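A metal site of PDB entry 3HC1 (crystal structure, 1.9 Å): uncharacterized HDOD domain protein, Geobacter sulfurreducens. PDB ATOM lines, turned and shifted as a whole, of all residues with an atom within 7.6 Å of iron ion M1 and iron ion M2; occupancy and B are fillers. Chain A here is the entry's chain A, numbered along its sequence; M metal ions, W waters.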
ATOM      1  N   LEU A 119      18.702  20.132  -6.423  1.00  0.00           N
ATOM      2  CA  LEU A 119      20.075  19.660  -6.384  1.00  0.00           C
ATOM      3  C   LEU A 119      20.318  18.600  -7.451  1.00  0.00           C
ATOM      4  O   LEU A 119      21.345  18.617  -8.092  1.00  0.00           O
ATOM      5  CB  LEU A 119      20.444  19.158  -4.973  1.00  0.00           C
ATOM      6  CG  LEU A 119      20.906  20.302  -4.038  1.00  0.00           C
ATOM      7  CD1 LEU A 119      19.868  21.424  -3.865  1.00  0.00           C
ATOM      8  CD2 LEU A 119      21.317  19.752  -2.687  1.00  0.00           C
ATOM      9  N   HIS A 122      20.269  20.203 -11.179  1.00  0.00           N
ATOM     10  CA  HIS A 122      21.522  20.948 -11.379  1.00  0.00           C
ATOM     11  C   HIS A 122      22.735  20.008 -11.569  1.00  0.00           C
ATOM     12  O   HIS A 122      23.608  20.236 -12.435  1.00  0.00           O
ATOM     13  CB  HIS A 122      21.771  21.861 -10.169  1.00  0.00           C
ATOM     14  CG  HIS A 122      23.147  22.458 -10.149  1.00  0.00           C
ATOM     15  ND1 HIS A 122      23.574  23.356 -11.105  1.00  0.00           N
ATOM     16  CD2 HIS A 122      24.209  22.244  -9.335  1.00  0.00           C
ATOM     17  CE1 HIS A 122      24.816  23.725 -10.834  1.00  0.00           C
ATOM     18  NE2 HIS A 122      25.234  23.047  -9.777  1.00  0.00           N
ATOM     19  N   SER A 123      22.795  18.964 -10.747  1.00  0.00           N
ATOM     20  CA  SER A 123      23.886  17.994 -10.783  1.00  0.00           C
ATOM     21  C   SER A 123      23.879  17.188 -12.076  1.00  0.00           C
ATOM     22  O   SER A 123      24.953  17.021 -12.725  1.00  0.00           O
ATOM     23  CB  SER A 123      23.855  17.077  -9.554  1.00  0.00           C
ATOM     24  OG  SER A 123      24.093  17.822  -8.348  1.00  0.00           O
ATOM     25  N   VAL A 126      24.970  19.610 -14.954  1.00  0.00           N
ATOM     26  CA  VAL A 126      26.406  19.735 -14.908  1.00  0.00           C
ATOM     27  C   VAL A 126      27.126  18.476 -15.453  1.00  0.00           C
ATOM     28  O   VAL A 126      28.051  18.604 -16.268  1.00  0.00           O
ATOM     29  CB  VAL A 126      26.919  20.160 -13.498  1.00  0.00           C
ATOM     30  CG1 VAL A 126      28.517  20.081 -13.370  1.00  0.00           C
ATOM     31  CG2 VAL A 126      26.406  21.604 -13.212  1.00  0.00           C
ATOM     32  N   GLY A 149      31.214  15.419 -12.625  1.00  0.00           N
ATOM     33  CA  GLY A 149      30.160  16.429 -12.721  1.00  0.00           C
ATOM     34  C   GLY A 149      28.945  16.150 -11.863  1.00  0.00           C
ATOM     35  O   GLY A 149      28.466  17.002 -11.099  1.00  0.00           O
ATOM     36  N   HIS A 152      29.786  16.737  -8.221  1.00  0.00           N
ATOM     37  CA  HIS A 152      30.471  17.994  -7.850  1.00  0.00           C
ATOM     38  C   HIS A 152      29.941  18.728  -6.593  1.00  0.00           C
ATOM     39  O   HIS A 152      30.687  19.243  -5.776  1.00  0.00           O
ATOM     40  CB  HIS A 152      30.641  18.950  -9.034  1.00  0.00           C
ATOM     41  CG  HIS A 152      29.435  19.809  -9.300  1.00  0.00           C
ATOM     42  ND1 HIS A 152      28.291  19.312  -9.869  1.00  0.00           N
ATOM     43  CD2 HIS A 152      29.186  21.133  -9.084  1.00  0.00           C
ATOM     44  CE1 HIS A 152      27.374  20.263  -9.940  1.00  0.00           C
ATOM     45  NE2 HIS A 152      27.901  21.383  -9.498  1.00  0.00           N
ATOM     46  N   ASP A 153      28.612  18.745  -6.474  1.00  0.00           N
ATOM     47  CA  ASP A 153      27.903  19.334  -5.382  1.00  0.00           C
ATOM     48  C   ASP A 153      27.423  18.339  -4.332  1.00  0.00           C
ATOM     49  O   ASP A 153      26.479  18.649  -3.567  1.00  0.00           O
ATOM     50  CB  ASP A 153      26.729  20.143  -5.939  1.00  0.00           C
ATOM     51  CG  ASP A 153      27.162  21.555  -6.348  1.00  0.00           C
ATOM     52  OD1 ASP A 153      28.263  21.969  -5.931  1.00  0.00           O
ATOM     53  OD2 ASP A 153      26.412  22.221  -7.107  1.00  0.00           O
ATOM     54  N   VAL A 154      28.062  17.170  -4.253  1.00  0.00           N
ATOM     55  CA  VAL A 154      27.647  16.177  -3.253  1.00  0.00           C
ATOM     56  C   VAL A 154      27.721  16.763  -1.810  1.00  0.00           C
ATOM     57  O   VAL A 154      26.965  16.386  -0.942  1.00  0.00           O
ATOM     58  CB  VAL A 154      28.456  14.856  -3.395  1.00  0.00           C
ATOM     59  CG1 VAL A 154      29.930  15.053  -2.974  1.00  0.00           C
ATOM     60  CG2 VAL A 154      27.837  13.778  -2.639  1.00  0.00           C
ATOM     61  N   GLU A 156      26.718  19.827  -0.935  1.00  0.00           N
ATOM     62  CA  GLU A 156      25.438  20.563  -0.725  1.00  0.00           C
ATOM     63  C   GLU A 156      24.356  19.575  -0.408  1.00  0.00           C
ATOM     64  O   GLU A 156      23.464  19.872   0.370  1.00  0.00           O
ATOM     65  CB  GLU A 156      24.976  21.375  -1.943  1.00  0.00           C
ATOM     66  CG  GLU A 156      25.826  22.500  -2.374  1.00  0.00           C
ATOM     67  CD  GLU A 156      25.720  23.719  -1.459  1.00  0.00           C
ATOM     68  OE1 GLU A 156      25.899  23.547  -0.250  1.00  0.00           O
ATOM     69  OE2 GLU A 156      25.478  24.825  -1.976  1.00  0.00           O
ATOM     70  N   PHE A 181      25.894  30.737  -2.560  1.00  0.00           N
ATOM     71  CA  PHE A 181      25.791  29.754  -1.495  1.00  0.00           C
ATOM     72  C   PHE A 181      27.164  29.534  -0.906  1.00  0.00           C
ATOM     73  O   PHE A 181      27.299  29.469   0.293  1.00  0.00           O
ATOM     74  CB  PHE A 181      25.204  28.455  -2.032  1.00  0.00           C
ATOM     75  CG  PHE A 181      23.701  28.383  -1.869  1.00  0.00           C
ATOM     76  CD1 PHE A 181      22.866  29.195  -2.621  1.00  0.00           C
ATOM     77  CD2 PHE A 181      23.142  27.458  -0.998  1.00  0.00           C
ATOM     78  CE1 PHE A 181      21.481  29.114  -2.480  1.00  0.00           C
ATOM     79  CE2 PHE A 181      21.759  27.386  -0.852  1.00  0.00           C
ATOM     80  CZ  PHE A 181      20.942  28.180  -1.604  1.00  0.00           C
ATOM     81  N   GLY A 182      28.182  29.421  -1.758  1.00  0.00           N
ATOM     82  CA  GLY A 182      29.528  29.225  -1.285  1.00  0.00           C
ATOM     83  C   GLY A 182      29.988  30.362  -0.356  1.00  0.00           C
ATOM     84  O   GLY A 182      30.681  30.103   0.637  1.00  0.00           O
ATOM     85  N   GLU A 185      27.964  30.011   2.918  1.00  0.00           N
ATOM     86  CA  GLU A 185      28.542  28.926   3.676  1.00  0.00           C
ATOM     87  C   GLU A 185      29.844  29.369   4.383  1.00  0.00           C
ATOM     88  O   GLU A 185      30.079  29.087   5.563  1.00  0.00           O
ATOM     89  CB  GLU A 185      28.790  27.710   2.745  1.00  0.00           C
ATOM     90  CG  GLU A 185      27.492  27.048   2.361  1.00  0.00           C
ATOM     91  CD  GLU A 185      27.608  26.129   1.179  1.00  0.00           C
ATOM     92  OE1 GLU A 185      28.736  25.857   0.662  1.00  0.00           O
ATOM     93  OE2 GLU A 185      26.526  25.759   0.706  1.00  0.00           O
ATOM     94  N   SER A 192      33.082  25.472   3.079  1.00  0.00           N
ATOM     95  CA  SER A 192      31.983  25.336   2.137  1.00  0.00           C
ATOM     96  C   SER A 192      31.696  23.878   1.719  1.00  0.00           C
ATOM     97  O   SER A 192      32.405  22.940   2.124  1.00  0.00           O
ATOM     98  CB  SER A 192      32.289  26.188   0.899  1.00  0.00           C
ATOM     99  OG  SER A 192      33.008  25.425  -0.070  1.00  0.00           O
ATOM    100  N   HIS A 193      30.691  23.705   0.881  1.00  0.00           N
ATOM    101  CA  HIS A 193      30.374  22.395   0.311  1.00  0.00           C
ATOM    102  C   HIS A 193      31.512  21.814  -0.527  1.00  0.00           C
ATOM    103  O   HIS A 193      31.529  20.576  -0.747  1.00  0.00           O
ATOM    104  CB  HIS A 193      29.096  22.423  -0.535  1.00  0.00           C
ATOM    105  CG  HIS A 193      29.216  23.227  -1.784  1.00  0.00           C
ATOM    106  ND1 HIS A 193      29.250  24.609  -1.784  1.00  0.00           N
ATOM    107  CD2 HIS A 193      29.364  22.852  -3.069  1.00  0.00           C
ATOM    108  CE1 HIS A 193      29.374  25.043  -3.021  1.00  0.00           C
ATOM    109  NE2 HIS A 193      29.417  23.988  -3.820  1.00  0.00           N
ATOM    110  N   CYS A 194      32.420  22.653  -1.024  1.00  0.00           N
ATOM    111  CA  CYS A 194      33.664  22.189  -1.678  1.00  0.00           C
ATOM    112  C   CYS A 194      34.487  21.347  -0.727  1.00  0.00           C
ATOM    113  O   CYS A 194      34.822  20.221  -1.017  1.00  0.00           O
ATOM    114  CB  CYS A 194      34.494  23.331  -2.181  1.00  0.00           C
ATOM    115  SG  CYS A 194      33.684  24.329  -3.462  1.00  0.00           S
ATOM    116  N   ILE A 214      35.434  18.186  -6.775  1.00  0.00           N
ATOM    117  CA  ILE A 214      34.504  18.648  -5.688  1.00  0.00           C
ATOM    118  C   ILE A 214      35.130  19.828  -4.918  1.00  0.00           C
ATOM    119  O   ILE A 214      34.467  20.821  -4.705  1.00  0.00           O
ATOM    120  CB  ILE A 214      34.129  17.469  -4.782  1.00  0.00           C
ATOM    121  CG1 ILE A 214      33.405  16.358  -5.536  1.00  0.00           C
ATOM    122  CG2 ILE A 214      33.224  17.918  -3.595  1.00  0.00           C
ATOM    123  CD1 ILE A 214      33.352  15.028  -4.699  1.00  0.00           C
ATOM    124  N   HIS A 217      35.879  23.150  -7.830  1.00  0.00           N
ATOM    125  CA  HIS A 217      34.954  23.463  -8.909  1.00  0.00           C
ATOM    126  C   HIS A 217      34.450  24.881  -8.957  1.00  0.00           C
ATOM    127  O   HIS A 217      33.949  25.286 -10.015  1.00  0.00           O
ATOM    128  CB  HIS A 217      33.803  22.482  -8.997  1.00  0.00           C
ATOM    129  CG  HIS A 217      32.781  22.622  -7.908  1.00  0.00           C
ATOM    130  ND1 HIS A 217      32.781  21.843  -6.768  1.00  0.00           N
ATOM    131  CD2 HIS A 217      31.651  23.368  -7.854  1.00  0.00           C
ATOM    132  CE1 HIS A 217      31.732  22.163  -6.027  1.00  0.00           C
ATOM    133  NE2 HIS A 217      31.091  23.146  -6.622  1.00  0.00           N
ATOM    134  N   HIS A 218      34.577  25.635  -7.862  1.00  0.00           N
ATOM    135  CA  HIS A 218      34.232  27.083  -7.860  1.00  0.00           C
ATOM    136  C   HIS A 218      35.427  27.988  -8.142  1.00  0.00           C
ATOM    137  O   HIS A 218      35.246  29.181  -8.225  1.00  0.00           O
ATOM    138  CB  HIS A 218      33.496  27.501  -6.556  1.00  0.00           C
ATOM    139  CG  HIS A 218      32.110  26.966  -6.461  1.00  0.00           C
ATOM    140  ND1 HIS A 218      31.067  27.518  -7.176  1.00  0.00           N
ATOM    141  CD2 HIS A 218      31.571  25.923  -5.756  1.00  0.00           C
ATOM    142  CE1 HIS A 218      29.968  26.803  -6.962  1.00  0.00           C
ATOM    143  NE2 HIS A 218      30.229  25.849  -6.087  1.00  0.00           N
ATOM    144  N   VAL A 234      34.153  20.571 -15.447  1.00  0.00           N
ATOM    145  CA  VAL A 234      33.036  20.598 -14.480  1.00  0.00           C
ATOM    146  C   VAL A 234      32.881  22.011 -13.940  1.00  0.00           C
ATOM    147  O   VAL A 234      31.732  22.468 -13.744  1.00  0.00           O
ATOM    148  CB  VAL A 234      33.254  19.563 -13.355  1.00  0.00           C
ATOM    149  CG1 VAL A 234      32.253  19.771 -12.099  1.00  0.00           C
ATOM    150  CG2 VAL A 234      33.229  18.099 -13.922  1.00  0.00           C
ATOM    151  N   ALA A 237      31.057  23.819 -16.646  1.00  0.00           N
ATOM    152  CA  ALA A 237      29.675  23.334 -16.699  1.00  0.00           C
ATOM    153  C   ALA A 237      28.809  23.857 -15.548  1.00  0.00           C
ATOM    154  O   ALA A 237      27.637  24.172 -15.740  1.00  0.00           O
ATOM    155  CB  ALA A 237      29.613  21.801 -16.814  1.00  0.00           C
ATOM    156  N   ASP A 238      29.393  24.004 -14.369  1.00  0.00           N
ATOM    157  CA  ASP A 238      28.661  24.482 -13.230  1.00  0.00           C
ATOM    158  C   ASP A 238      28.287  25.954 -13.417  1.00  0.00           C
ATOM    159  O   ASP A 238      27.118  26.341 -13.257  1.00  0.00           O
ATOM    160  CB  ASP A 238      29.442  24.297 -11.924  1.00  0.00           C
ATOM    161  CG  ASP A 238      28.791  24.989 -10.789  1.00  0.00           C
ATOM    162  OD1 ASP A 238      27.638  24.657 -10.528  1.00  0.00           O
ATOM    163  OD2 ASP A 238      29.370  25.903 -10.175  1.00  0.00           O
ATOM    164  N   GLU A 239      29.268  26.775 -13.772  1.00  0.00           N
ATOM    165  CA  GLU A 239      29.004  28.185 -14.029  1.00  0.00           C
ATOM    166  C   GLU A 239      27.982  28.381 -15.185  1.00  0.00           C
ATOM    167  O   GLU A 239      27.037  29.183 -15.077  1.00  0.00           O
ATOM    168  CB  GLU A 239      30.318  28.959 -14.262  1.00  0.00           C
ATOM    169  CG  GLU A 239      30.062  30.472 -14.231  1.00  0.00           C
ATOM    170  CD  GLU A 239      31.275  31.292 -14.025  1.00  0.00           C
ATOM    171  OE1 GLU A 239      32.338  30.738 -14.259  1.00  0.00           O
ATOM    172  OE2 GLU A 239      31.179  32.473 -13.611  1.00  0.00           O
ATOM    173  N   CYS A 241      25.574  26.196 -16.200  1.00  0.00           N
ATOM    174  CA  CYS A 241      24.281  25.802 -15.672  1.00  0.00           C
ATOM    175  C   CYS A 241      23.691  26.856 -14.752  1.00  0.00           C
ATOM    176  O   CYS A 241      22.522  27.165 -14.863  1.00  0.00           O
ATOM    177  CB  CYS A 241      24.365  24.470 -14.988  1.00  0.00           C
ATOM    178  SG  CYS A 241      24.484  23.118 -16.213  1.00  0.00           S
ATOM    179  N   THR A 242      24.522  27.442 -13.877  1.00  0.00           N
ATOM    180  CA  THR A 242      24.063  28.447 -12.924  1.00  0.00           C
ATOM    181  C   THR A 242      23.587  29.679 -13.670  1.00  0.00           C
ATOM    182  O   THR A 242      22.590  30.276 -13.289  1.00  0.00           O
ATOM    183  CB  THR A 242      25.170  28.790 -11.924  1.00  0.00           C
ATOM    184  OG1 THR A 242      25.550  27.575 -11.271  1.00  0.00           O
ATOM    185  CG2 THR A 242      24.695  29.816 -10.847  1.00  0.00           C
ATOM    186  N   LEU A 246      19.834  26.459 -14.826  1.00  0.00           N
ATOM    187  CA  LEU A 246      19.915  25.053 -14.436  1.00  0.00           C
ATOM    188  C   LEU A 246      20.741  24.941 -13.130  1.00  0.00           C
ATOM    189  O   LEU A 246      21.678  24.170 -13.022  1.00  0.00           O
ATOM    190  CB  LEU A 246      20.476  24.231 -15.596  1.00  0.00           C
ATOM    191  CG  LEU A 246      20.496  22.689 -15.588  1.00  0.00           C
ATOM    192  CD1 LEU A 246      19.185  22.146 -15.052  1.00  0.00           C
ATOM    193  CD2 LEU A 246      20.839  22.189 -16.978  1.00  0.00           C
ATOM    194  N   GLY A 247      20.421  25.800 -12.173  1.00  0.00           N
ATOM    195  CA  GLY A 247      21.160  25.873 -10.918  1.00  0.00           C
ATOM    196  C   GLY A 247      20.485  26.623  -9.803  1.00  0.00           C
ATOM    197  O   GLY A 247      19.286  27.023  -9.887  1.00  0.00           O
ATOM    198  N   PHE A 248      21.219  26.778  -8.722  1.00  0.00           N
ATOM    199  CA  PHE A 248      20.627  27.394  -7.520  1.00  0.00           C
ATOM    200  C   PHE A 248      21.636  28.142  -6.688  1.00  0.00           C
ATOM    201  O   PHE A 248      21.262  28.758  -5.714  1.00  0.00           O
ATOM    202  CB  PHE A 248      19.976  26.292  -6.621  1.00  0.00           C
ATOM    203  CG  PHE A 248      20.981  25.297  -6.062  1.00  0.00           C
ATOM    204  CD1 PHE A 248      21.413  24.254  -6.834  1.00  0.00           C
ATOM    205  CD2 PHE A 248      21.535  25.456  -4.776  1.00  0.00           C
ATOM    206  CE1 PHE A 248      22.396  23.333  -6.357  1.00  0.00           C
ATOM    207  CE2 PHE A 248      22.486  24.573  -4.285  1.00  0.00           C
ATOM    208  CZ  PHE A 248      22.921  23.503  -5.075  1.00  0.00           C
ATOM    209  N   GLU A 249      22.940  27.985  -6.975  1.00  0.00           N
ATOM    210  CA  GLU A 249      23.944  28.435  -6.031  1.00  0.00           C
ATOM    211  C   GLU A 249      24.187  29.918  -6.129  1.00  0.00           C
ATOM    212  O   GLU A 249      24.853  30.474  -5.280  1.00  0.00           O
ATOM    213  CB  GLU A 249      25.256  27.651  -6.241  1.00  0.00           C
ATOM    214  CG  GLU A 249      25.122  26.169  -5.880  1.00  0.00           C
ATOM    215  CD  GLU A 249      26.189  25.374  -6.535  1.00  0.00           C
ATOM    216  OE1 GLU A 249      26.095  25.169  -7.740  1.00  0.00           O
ATOM    217  OE2 GLU A 249      27.160  25.010  -5.845  1.00  0.00           O
HETATM  218 FE    FE M   1      29.126  23.956  -6.099  1.00  0.00          FE
HETATM  219 FE    FE M   2      27.137  23.431  -8.700  1.00  0.00          FE
HETATM  220  O   HOH W   1      28.863  24.077  -7.970  1.00  0.00           O
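A ring nitrogen (ND1) of His 152 lies within hydrogen-bond range of the backbone carbonyl oxygen of Gly 149, 2.6 Å away.
The side-chain hydroxyl of Thr 242 lies within hydrogen-bond range of the backbone carbonyl oxygen of Asp 238, at 2.8 Å.
N of Phe 181 sits at hydrogen-bond distance from O of Glu 249 (2.9 Å).
OE1 of Glu 185 lies within hydrogen-bond range of ND1 of His 193.
ND1 of His 217 lies close to O of His 152.
A ring nitrogen (ND1) of His 217 sits at hydrogen-bond distance from the backbone carbonyl oxygen of Ile 214 (2.9 Å).
A ring nitrogen (ND1) of His 122 sits at hydrogen-bond distance from the backbone carbonyl oxygen (O) of Leu 246 (2.8 Å).
Of the 28 residues printed, 5 come within 4 Å of iron ion M2.
Iron ion M1 is bound by water W1 (1.9 Å), the side-chain carboxylate (OD1) of Asp 153 (2.2 Å), a ring nitrogen (NE2) of His 217 (2.2 Å), a ring nitrogen (NE2) of His 218 (2.2 Å), the side-chain carboxylate (OE2) of Glu 249 (2.2 Å) and a ring nitrogen (NE2) of His 193 (2.3 Å).
Iron ion M2 is bound by water W1 (2.0 Å), the side-chain carboxylate of Asp 153 (2.1 Å), a ring nitrogen (NE2) of His 122 (2.2 Å), the side-chain carboxylate of Glu 249 (2.2 Å), the side-chain carboxylate of Asp 238 (2.3 Å) and a ring nitrogen (NE2) of His 152 (2.3 Å).
Iron ion M2 has six donor atoms within binding distance.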
